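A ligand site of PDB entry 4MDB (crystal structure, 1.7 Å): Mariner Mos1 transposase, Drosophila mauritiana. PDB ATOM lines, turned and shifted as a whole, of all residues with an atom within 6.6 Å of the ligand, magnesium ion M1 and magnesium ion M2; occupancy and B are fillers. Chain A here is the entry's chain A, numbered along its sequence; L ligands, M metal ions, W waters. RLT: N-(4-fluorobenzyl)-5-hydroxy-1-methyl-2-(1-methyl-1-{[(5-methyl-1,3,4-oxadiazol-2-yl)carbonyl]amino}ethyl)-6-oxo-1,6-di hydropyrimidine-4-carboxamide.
OH of Tyr 156 sits at hydrogen-bond distance from NAO of the ligand (3.3 Å).
OE1 of Glu 37 sits at hydrogen-bond distance from NE2 of His 134 (2.7 Å). The backbone carbonyl oxygen (O) of Ala 155 sits at hydrogen-bond distance from the side-chain hydroxyl (OG) of Ser 157, 3.0 Å away. The backbone carbonyl oxygen (O) of Asp 129 lies within hydrogen-bond range of a ring nitrogen (ND1) of His 134, 2.8 Å away. The side-chain carboxylate of Asp 129 sits close to the backbone NH of Ala 131, at 3.3 Å. O of Tyr 156 is in hydrogen-bond range of OH of Tyr 223 (2.8 Å).
O of Asn 130 sits close to FAI of the ligand (3.5 Å). Merely in contact with the ligand: Ala 155 (3.5 Å) and Ala 131 (3.6 Å). Hydrophobic or aromatic side chains that line the ligand: Ala 155 and Tyr 156. Of the 22 residues printed, 7 come within 4 Å of the ligand. The nearest printed residue that does not touch the ligand is Pro 158 (4.02 Å).
The nearest printed residue that does not touch magnesium ion M1 is Glu 37 (4.1 Å).
Glu 37 touches magnesium ion M2. Within 4 Å of magnesium ion M2: Asp 36, Glu 37 and Asp 129. The nearest printed residue that does not touch magnesium ion M2 is Asp 164 (4.8 Å).
OD2 of Asp 36 binds magnesium ion M1 (1.9 Å). Water W3 is bound to magnesium ion M1 (2.0 Å). Magnesium ion M1 is bound by OAH of the ligand, 2.0 Å away. Magnesium ion M1 is bound by OD1 of Asp 164 (2.1 Å). An oxygen (OAG) of the ligand binds magnesium ion M1, 2.1 Å away. Magnesium ion M1 is bound by OD2 of Asp 164 (2.3 Å).
Magnesium ion M2 is bound by an oxygen (OAE) of the ligand (2.0 Å), the side-chain carboxylate (OD1) of Asp 36 (2.1 Å), the side-chain carboxylate (OD2) of Asp 129 (2.1 Å), water W4 (2.1 Å), water W2 (2.1 Å) and an oxygen (OAH) of the ligand (2.1 Å). Magnesium ion M2 has six donor atoms within binding distance.
Water W4 bridges the side-chain carboxylate (OE2) of Glu 37 (2.6 Å) and the side-chain carboxylate (OD1) of Asp 129 (2.8 Å).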
ATOM      1  N   HIS A   2       1.570  -6.237  -2.614  1.00  0.00           N
ATOM      2  CA  HIS A   2       0.168  -5.873  -2.217  1.00  0.00           C
ATOM      3  C   HIS A   2      -0.555  -7.064  -1.573  1.00  0.00           C
ATOM      4  O   HIS A   2      -0.664  -8.130  -2.175  1.00  0.00           O
ATOM      5  CB  HIS A   2      -0.618  -5.397  -3.452  1.00  0.00           C
ATOM      6  CG  HIS A   2      -1.919  -4.721  -3.128  1.00  0.00           C
ATOM      7  ND1 HIS A   2      -1.992  -3.432  -2.647  1.00  0.00           N
ATOM      8  CD2 HIS A   2      -3.196  -5.160  -3.238  1.00  0.00           C
ATOM      9  CE1 HIS A   2      -3.260  -3.102  -2.467  1.00  0.00           C
ATOM     10  NE2 HIS A   2      -4.013  -4.139  -2.812  1.00  0.00           N
ATOM     11  N   GLN A   8     -11.165  -8.185  -3.259  1.00  0.00           N
ATOM     12  CA  GLN A   8     -10.218  -8.350  -4.390  1.00  0.00           C
ATOM     13  C   GLN A   8     -10.008  -9.824  -4.747  1.00  0.00           C
ATOM     14  O   GLN A   8      -9.936 -10.195  -5.945  1.00  0.00           O
ATOM     15  CB  GLN A   8      -8.911  -7.678  -4.105  1.00  0.00           C
ATOM     16  CG  GLN A   8      -9.018  -6.136  -3.949  1.00  0.00           C
ATOM     17  CD  GLN A   8      -7.870  -5.484  -3.211  1.00  0.00           C
ATOM     18  OE1 GLN A   8      -7.004  -6.136  -2.669  1.00  0.00           O
ATOM     19  NE2 GLN A   8      -7.896  -4.155  -3.151  1.00  0.00           N
ATOM     20  N   ARG A  11     -13.275 -11.197  -6.365  1.00  0.00           N
ATOM     21  CA  ARG A  11     -13.416 -10.721  -7.783  1.00  0.00           C
ATOM     22  C   ARG A  11     -12.471 -11.508  -8.694  1.00  0.00           C
ATOM     23  O   ARG A  11     -12.881 -12.041  -9.789  1.00  0.00           O
ATOM     24  CB  ARG A  11     -13.143  -9.229  -7.905  1.00  0.00           C
ATOM     25  CG  ARG A  11     -13.393  -8.695  -9.342  1.00  0.00           C
ATOM     26  CD  ARG A  11     -14.039  -7.314  -9.303  1.00  0.00           C
ATOM     27  NE  ARG A  11     -14.023  -6.575 -10.590  1.00  0.00           N
ATOM     28  CZ  ARG A  11     -13.280  -5.496 -10.887  1.00  0.00           C
ATOM     29  NH1 ARG A  11     -12.404  -4.988 -10.018  1.00  0.00           N
ATOM     30  NH2 ARG A  11     -13.402  -4.958 -12.093  1.00  0.00           N
ATOM     31  N   GLY A  35      -3.491  -5.410 -24.193  1.00  0.00           N
ATOM     32  CA  GLY A  35      -2.564  -4.295 -24.147  1.00  0.00           C
ATOM     33  C   GLY A  35      -2.470  -3.697 -22.795  1.00  0.00           C
ATOM     34  O   GLY A  35      -3.300  -3.947 -21.886  1.00  0.00           O
ATOM     35  N   ASP A  36      -1.472  -2.860 -22.642  1.00  0.00           N
ATOM     36  CA  ASP A  36      -1.188  -2.221 -21.314  1.00  0.00           C
ATOM     37  C   ASP A  36      -0.077  -1.170 -21.559  1.00  0.00           C
ATOM     38  O   ASP A  36       0.628  -1.145 -22.588  1.00  0.00           O
ATOM     39  CB  ASP A  36      -0.660  -3.264 -20.330  1.00  0.00           C
ATOM     40  CG  ASP A  36      -0.623  -2.785 -18.881  1.00  0.00           C
ATOM     41  OD1 ASP A  36      -1.503  -1.995 -18.530  1.00  0.00           O
ATOM     42  OD2 ASP A  36       0.314  -3.324 -18.217  1.00  0.00           O
ATOM     43  N   GLU A  37       0.083  -0.308 -20.545  1.00  0.00           N
ATOM     44  CA  GLU A  37       1.029   0.784 -20.513  1.00  0.00           C
ATOM     45  C   GLU A  37       2.169   0.448 -19.552  1.00  0.00           C
ATOM     46  O   GLU A  37       1.951  -0.135 -18.492  1.00  0.00           O
ATOM     47  CB  GLU A  37       0.298   2.047 -20.036  1.00  0.00           C
ATOM     48  CG  GLU A  37      -0.817   2.536 -20.926  1.00  0.00           C
ATOM     49  CD  GLU A  37      -2.235   2.021 -20.564  1.00  0.00           C
ATOM     50  OE1 GLU A  37      -3.236   2.663 -21.035  1.00  0.00           O
ATOM     51  OE2 GLU A  37      -2.325   0.993 -19.843  1.00  0.00           O
ATOM     52  N   LYS A  38       3.368   0.885 -19.877  1.00  0.00           N
ATOM     53  CA  LYS A  38       4.552   0.792 -18.984  1.00  0.00           C
ATOM     54  C   LYS A  38       5.483   2.001 -19.188  1.00  0.00           C
ATOM     55  O   LYS A  38       5.715   2.398 -20.319  1.00  0.00           O
ATOM     56  CB  LYS A  38       5.328  -0.485 -19.302  1.00  0.00           C
ATOM     57  CG  LYS A  38       6.652  -0.684 -18.606  1.00  0.00           C
ATOM     58  CD  LYS A  38       7.176  -2.082 -18.812  1.00  0.00           C
ATOM     59  CE  LYS A  38       8.537  -2.314 -18.140  1.00  0.00           C
ATOM     60  NZ  LYS A  38       8.445  -2.102 -16.654  1.00  0.00           N
ATOM     61  N   ASP A 129      -6.691  -3.668 -18.676  1.00  0.00           N
ATOM     62  CA  ASP A 129      -6.990  -3.499 -17.258  1.00  0.00           C
ATOM     63  C   ASP A 129      -7.924  -2.334 -16.911  1.00  0.00           C
ATOM     64  O   ASP A 129      -8.418  -1.630 -17.774  1.00  0.00           O
ATOM     65  CB  ASP A 129      -5.695  -3.565 -16.480  1.00  0.00           C
ATOM     66  CG  ASP A 129      -4.787  -2.356 -16.624  1.00  0.00           C
ATOM     67  OD1 ASP A 129      -5.300  -1.302 -16.914  1.00  0.00           O
ATOM     68  OD2 ASP A 129      -3.495  -2.462 -16.503  1.00  0.00           O
ATOM     69  N   ASN A 130      -8.162  -2.167 -15.608  1.00  0.00           N
ATOM     70  CA  ASN A 130      -9.162  -1.228 -15.116  1.00  0.00           C
ATOM     71  C   ASN A 130      -8.689   0.161 -14.798  1.00  0.00           C
ATOM     72  O   ASN A 130      -9.313   0.837 -13.995  1.00  0.00           O
ATOM     73  CB  ASN A 130      -9.836  -1.772 -13.844  1.00  0.00           C
ATOM     74  CG  ASN A 130     -10.421  -3.112 -14.054  1.00  0.00           C
ATOM     75  OD1 ASN A 130     -11.461  -3.231 -14.710  1.00  0.00           O
ATOM     76  ND2 ASN A 130      -9.683  -4.149 -13.624  1.00  0.00           N
ATOM     77  N   ALA A 131      -7.605   0.597 -15.403  1.00  0.00           N
ATOM     78  CA  ALA A 131      -7.163   1.957 -15.343  1.00  0.00           C
ATOM     79  C   ALA A 131      -8.331   2.849 -15.705  1.00  0.00           C
ATOM     80  O   ALA A 131      -9.146   2.540 -16.565  1.00  0.00           O
ATOM     81  CB  ALA A 131      -5.993   2.224 -16.234  1.00  0.00           C
ATOM     82  N   PRO A 132      -8.482   3.940 -14.931  1.00  0.00           N
ATOM     83  CA  PRO A 132      -9.658   4.818 -15.181  1.00  0.00           C
ATOM     84  C   PRO A 132      -9.858   5.271 -16.622  1.00  0.00           C
ATOM     85  O   PRO A 132     -11.009   5.264 -17.083  1.00  0.00           O
ATOM     86  CB  PRO A 132      -9.412   6.022 -14.244  1.00  0.00           C
ATOM     87  CG  PRO A 132      -8.645   5.419 -13.134  1.00  0.00           C
ATOM     88  CD  PRO A 132      -7.729   4.320 -13.725  1.00  0.00           C
ATOM     89  N   HIS A 134      -9.293   3.677 -19.150  1.00  0.00           N
ATOM     90  CA  HIS A 134      -9.805   2.459 -19.865  1.00  0.00           C
ATOM     91  C   HIS A 134     -11.320   2.256 -19.682  1.00  0.00           C
ATOM     92  O   HIS A 134     -11.927   1.488 -20.419  1.00  0.00           O
ATOM     93  CB  HIS A 134      -9.091   1.203 -19.364  1.00  0.00           C
ATOM     94  CG  HIS A 134      -7.630   1.157 -19.680  1.00  0.00           C
ATOM     95  ND1 HIS A 134      -6.878   0.020 -19.476  1.00  0.00           N
ATOM     96  CD2 HIS A 134      -6.794   2.059 -20.209  1.00  0.00           C
ATOM     97  CE1 HIS A 134      -5.650   0.230 -19.872  1.00  0.00           C
ATOM     98  NE2 HIS A 134      -5.564   1.477 -20.290  1.00  0.00           N
ATOM     99  N   ALA A 154     -10.157  -8.401 -13.210  1.00  0.00           N
ATOM    100  CA  ALA A 154     -10.079  -7.949 -11.826  1.00  0.00           C
ATOM    101  C   ALA A 154      -8.958  -6.969 -11.526  1.00  0.00           C
ATOM    102  O   ALA A 154      -7.817  -7.081 -11.979  1.00  0.00           O
ATOM    103  CB  ALA A 154      -9.929  -9.163 -10.932  1.00  0.00           C
ATOM    104  N   ALA A 155      -9.257  -6.029 -10.647  1.00  0.00           N
ATOM    105  CA  ALA A 155      -8.234  -5.178 -10.047  1.00  0.00           C
ATOM    106  C   ALA A 155      -7.009  -5.901  -9.415  1.00  0.00           C
ATOM    107  O   ALA A 155      -7.142  -7.034  -8.948  1.00  0.00           O
ATOM    108  CB  ALA A 155      -8.941  -4.296  -9.031  1.00  0.00           C
ATOM    109  N   TYR A 156      -5.844  -5.263  -9.462  1.00  0.00           N
ATOM    110  CA  TYR A 156      -4.595  -5.750  -8.929  1.00  0.00           C
ATOM    111  C   TYR A 156      -4.265  -7.135  -9.474  1.00  0.00           C
ATOM    112  O   TYR A 156      -3.731  -7.974  -8.734  1.00  0.00           O
ATOM    113  CB  TYR A 156      -4.639  -5.796  -7.388  1.00  0.00           C
ATOM    114  CG  TYR A 156      -4.632  -4.431  -6.784  1.00  0.00           C
ATOM    115  CD1 TYR A 156      -3.428  -3.770  -6.551  1.00  0.00           C
ATOM    116  CD2 TYR A 156      -5.813  -3.781  -6.493  1.00  0.00           C
ATOM    117  CE1 TYR A 156      -3.407  -2.496  -6.008  1.00  0.00           C
ATOM    118  CE2 TYR A 156      -5.809  -2.510  -5.944  1.00  0.00           C
ATOM    119  CZ  TYR A 156      -4.618  -1.867  -5.710  1.00  0.00           C
ATOM    120  OH  TYR A 156      -4.623  -0.608  -5.179  1.00  0.00           O
ATOM    121  N   SER A 157      -4.521  -7.365 -10.784  1.00  0.00           N
ATOM    122  CA  SER A 157      -4.250  -8.694 -11.337  1.00  0.00           C
ATOM    123  C   SER A 157      -3.263  -8.700 -12.533  1.00  0.00           C
ATOM    124  O   SER A 157      -3.558  -9.191 -13.573  1.00  0.00           O
ATOM    125  CB  SER A 157      -5.559  -9.319 -11.704  1.00  0.00           C
ATOM    126  OG  SER A 157      -6.463  -9.479 -10.565  1.00  0.00           O
ATOM    127  N   PRO A 158      -2.081  -8.112 -12.364  1.00  0.00           N
ATOM    128  CA  PRO A 158      -1.114  -8.253 -13.493  1.00  0.00           C
ATOM    129  C   PRO A 158      -0.627  -9.663 -13.746  1.00  0.00           C
ATOM    130  O   PRO A 158      -0.203  -9.974 -14.844  1.00  0.00           O
ATOM    131  CB  PRO A 158       0.016  -7.330 -13.058  1.00  0.00           C
ATOM    132  CG  PRO A 158      -0.017  -7.392 -11.553  1.00  0.00           C
ATOM    133  CD  PRO A 158      -1.460  -7.389 -11.214  1.00  0.00           C
ATOM    134  N   ALA A 161      -2.780 -10.638 -16.529  1.00  0.00           N
ATOM    135  CA  ALA A 161      -2.675  -9.780 -17.730  1.00  0.00           C
ATOM    136  C   ALA A 161      -1.455 -10.206 -18.555  1.00  0.00           C
ATOM    137  O   ALA A 161      -0.301 -10.053 -18.129  1.00  0.00           O
ATOM    138  CB  ALA A 161      -2.521  -8.341 -17.303  1.00  0.00           C
ATOM    139  N   SER A 163       0.216  -8.860 -20.927  1.00  0.00           N
ATOM    140  CA  SER A 163       1.196  -7.799 -21.093  1.00  0.00           C
ATOM    141  C   SER A 163       2.123  -7.710 -19.909  1.00  0.00           C
ATOM    142  O   SER A 163       3.328  -7.473 -20.116  1.00  0.00           O
ATOM    143  CB  SER A 163       0.564  -6.452 -21.345  1.00  0.00           C
ATOM    144  OG  SER A 163      -0.303  -6.421 -22.504  1.00  0.00           O
ATOM    145  N   ASP A 164       1.571  -7.948 -18.707  1.00  0.00           N
ATOM    146  CA  ASP A 164       2.428  -7.915 -17.496  1.00  0.00           C
ATOM    147  C   ASP A 164       3.180  -9.210 -17.238  1.00  0.00           C
ATOM    148  O   ASP A 164       4.412  -9.172 -17.104  1.00  0.00           O
ATOM    149  CB  ASP A 164       1.537  -7.496 -16.317  1.00  0.00           C
ATOM    150  CG  ASP A 164       1.203  -5.999 -16.397  1.00  0.00           C
ATOM    151  OD1 ASP A 164       2.138  -5.191 -16.706  1.00  0.00           O
ATOM    152  OD2 ASP A 164       0.086  -5.599 -16.187  1.00  0.00           O
ATOM    153  N   PHE A 168       5.956  -7.666 -20.760  1.00  0.00           N
ATOM    154  CA  PHE A 168       6.777  -6.688 -19.983  1.00  0.00           C
ATOM    155  C   PHE A 168       7.714  -7.426 -19.017  1.00  0.00           C
ATOM    156  O   PHE A 168       8.780  -6.903 -18.737  1.00  0.00           O
ATOM    157  CB  PHE A 168       5.907  -5.759 -19.211  1.00  0.00           C
ATOM    158  CG  PHE A 168       5.113  -4.775 -20.044  1.00  0.00           C
ATOM    159  CD1 PHE A 168       5.497  -4.391 -21.380  1.00  0.00           C
ATOM    160  CD2 PHE A 168       3.977  -4.251 -19.545  1.00  0.00           C
ATOM    161  CE1 PHE A 168       4.735  -3.498 -22.073  1.00  0.00           C
ATOM    162  CE2 PHE A 168       3.197  -3.380 -20.250  1.00  0.00           C
ATOM    163  CZ  PHE A 168       3.606  -2.967 -21.548  1.00  0.00           C
ATOM    164  N   TYR A 223      -2.787 -14.384  -4.869  1.00  0.00           N
ATOM    165  CA  TYR A 223      -1.626 -14.534  -5.766  1.00  0.00           C
ATOM    166  C   TYR A 223      -1.117 -15.930  -5.671  1.00  0.00           C
ATOM    167  O   TYR A 223      -1.428 -16.636  -4.710  1.00  0.00           O
ATOM    168  CB  TYR A 223      -0.515 -13.519  -5.490  1.00  0.00           C
ATOM    169  CG  TYR A 223      -0.938 -12.108  -5.764  1.00  0.00           C
ATOM    170  CD1 TYR A 223      -1.512 -11.754  -6.976  1.00  0.00           C
ATOM    171  CD2 TYR A 223      -0.822 -11.126  -4.797  1.00  0.00           C
ATOM    172  CE1 TYR A 223      -1.932 -10.465  -7.216  1.00  0.00           C
ATOM    173  CE2 TYR A 223      -1.221  -9.843  -5.033  1.00  0.00           C
ATOM    174  CZ  TYR A 223      -1.763  -9.497  -6.250  1.00  0.00           C
ATOM    175  OH  TYR A 223      -2.171  -8.244  -6.445  1.00  0.00           O
HETATM  176  CAA RLT L   1      -6.861  -1.494  -8.955  1.00  0.00           C
HETATM  177  CAB RLT L   1       2.050  -3.900 -11.950  1.00  0.00           C
HETATM  178  CAC RLT L   1       0.257  -3.563  -9.496  1.00  0.00           C
HETATM  179  CAD RLT L   1       1.550  -1.188  -9.988  1.00  0.00           C
HETATM  180  OAE RLT L   1      -2.388  -0.421 -14.828  1.00  0.00           O
HETATM  181  OAF RLT L   1      -2.596  -2.964 -10.273  1.00  0.00           O
HETATM  182  OAG RLT L   1       1.448  -3.803 -14.357  1.00  0.00           O
HETATM  183  OAH RLT L   1      -0.532  -2.420 -15.510  1.00  0.00           O
HETATM  184  FAI RLT L   1      -8.425  -0.552 -10.937  1.00  0.00           F
HETATM  185  CAJ RLT L   1      -6.504  -0.834 -12.337  1.00  0.00           C
HETATM  186  CAK RLT L   1      -6.722   1.144 -11.014  1.00  0.00           C
HETATM  187  CAL RLT L   1      -5.276  -0.370 -12.830  1.00  0.00           C
HETATM  188  CAM RLT L   1      -5.496   1.621 -11.503  1.00  0.00           C
HETATM  189  CAN RLT L   1      -3.420   1.416 -12.891  1.00  0.00           C
HETATM  190  NAO RLT L   1      -4.938   0.239  -8.364  1.00  0.00           N
HETATM  191  NAP RLT L   1      -3.536   0.120  -8.589  1.00  0.00           N
HETATM  192  NAQ RLT L   1      -0.881  -1.419 -11.900  1.00  0.00           N
HETATM  193  NAR RLT L   1      -2.443   0.345 -12.661  1.00  0.00           N
HETATM  194  NAS RLT L   1      -0.995  -1.421  -9.546  1.00  0.00           N
HETATM  195  OAT RLT L   1      -4.572  -1.744  -9.368  1.00  0.00           O
HETATM  196  CAU RLT L   1      -2.123  -0.518 -13.661  1.00  0.00           C
HETATM  197  CAV RLT L   1      -2.255  -1.899  -9.741  1.00  0.00           C
HETATM  198  CAW RLT L   1      -5.485  -0.904  -8.855  1.00  0.00           C
HETATM  199  CAX RLT L   1      -7.242  -0.079 -11.428  1.00  0.00           C
HETATM  200  CAY RLT L   1      -4.757   0.883 -12.417  1.00  0.00           C
HETATM  201  CAZ RLT L   1      -0.348  -2.230 -14.199  1.00  0.00           C
HETATM  202  CBA RLT L   1      -3.380  -1.080  -9.225  1.00  0.00           C
HETATM  203  CBB RLT L   1      -1.145  -1.454 -13.265  1.00  0.00           C
HETATM  204  CBC RLT L   1       0.106  -2.190 -11.380  1.00  0.00           C
HETATM  205  CBD RLT L   1       0.679  -3.079 -13.652  1.00  0.00           C
HETATM  206  NBE RLT L   1       0.899  -2.989 -12.268  1.00  0.00           N
HETATM  207  CBF RLT L   1       0.280  -2.069  -9.780  1.00  0.00           C
HETATM  208 MG    MG M   1       0.956  -3.509 -16.396  1.00  0.00          MG
HETATM  209 MG    MG M   2      -1.837  -1.211 -16.636  1.00  0.00          MG
HETATM  210  O   HOH W   1      -6.637  -3.896 -13.080  1.00  0.00           O
HETATM  211  O   HOH W   2      -0.272   0.167 -16.901  1.00  0.00           O
HETATM  212  O   HOH W   3       2.395  -2.079 -16.643  1.00  0.00           O
HETATM  213  O   HOH W   4      -3.052   0.268 -17.461  1.00  0.00           O
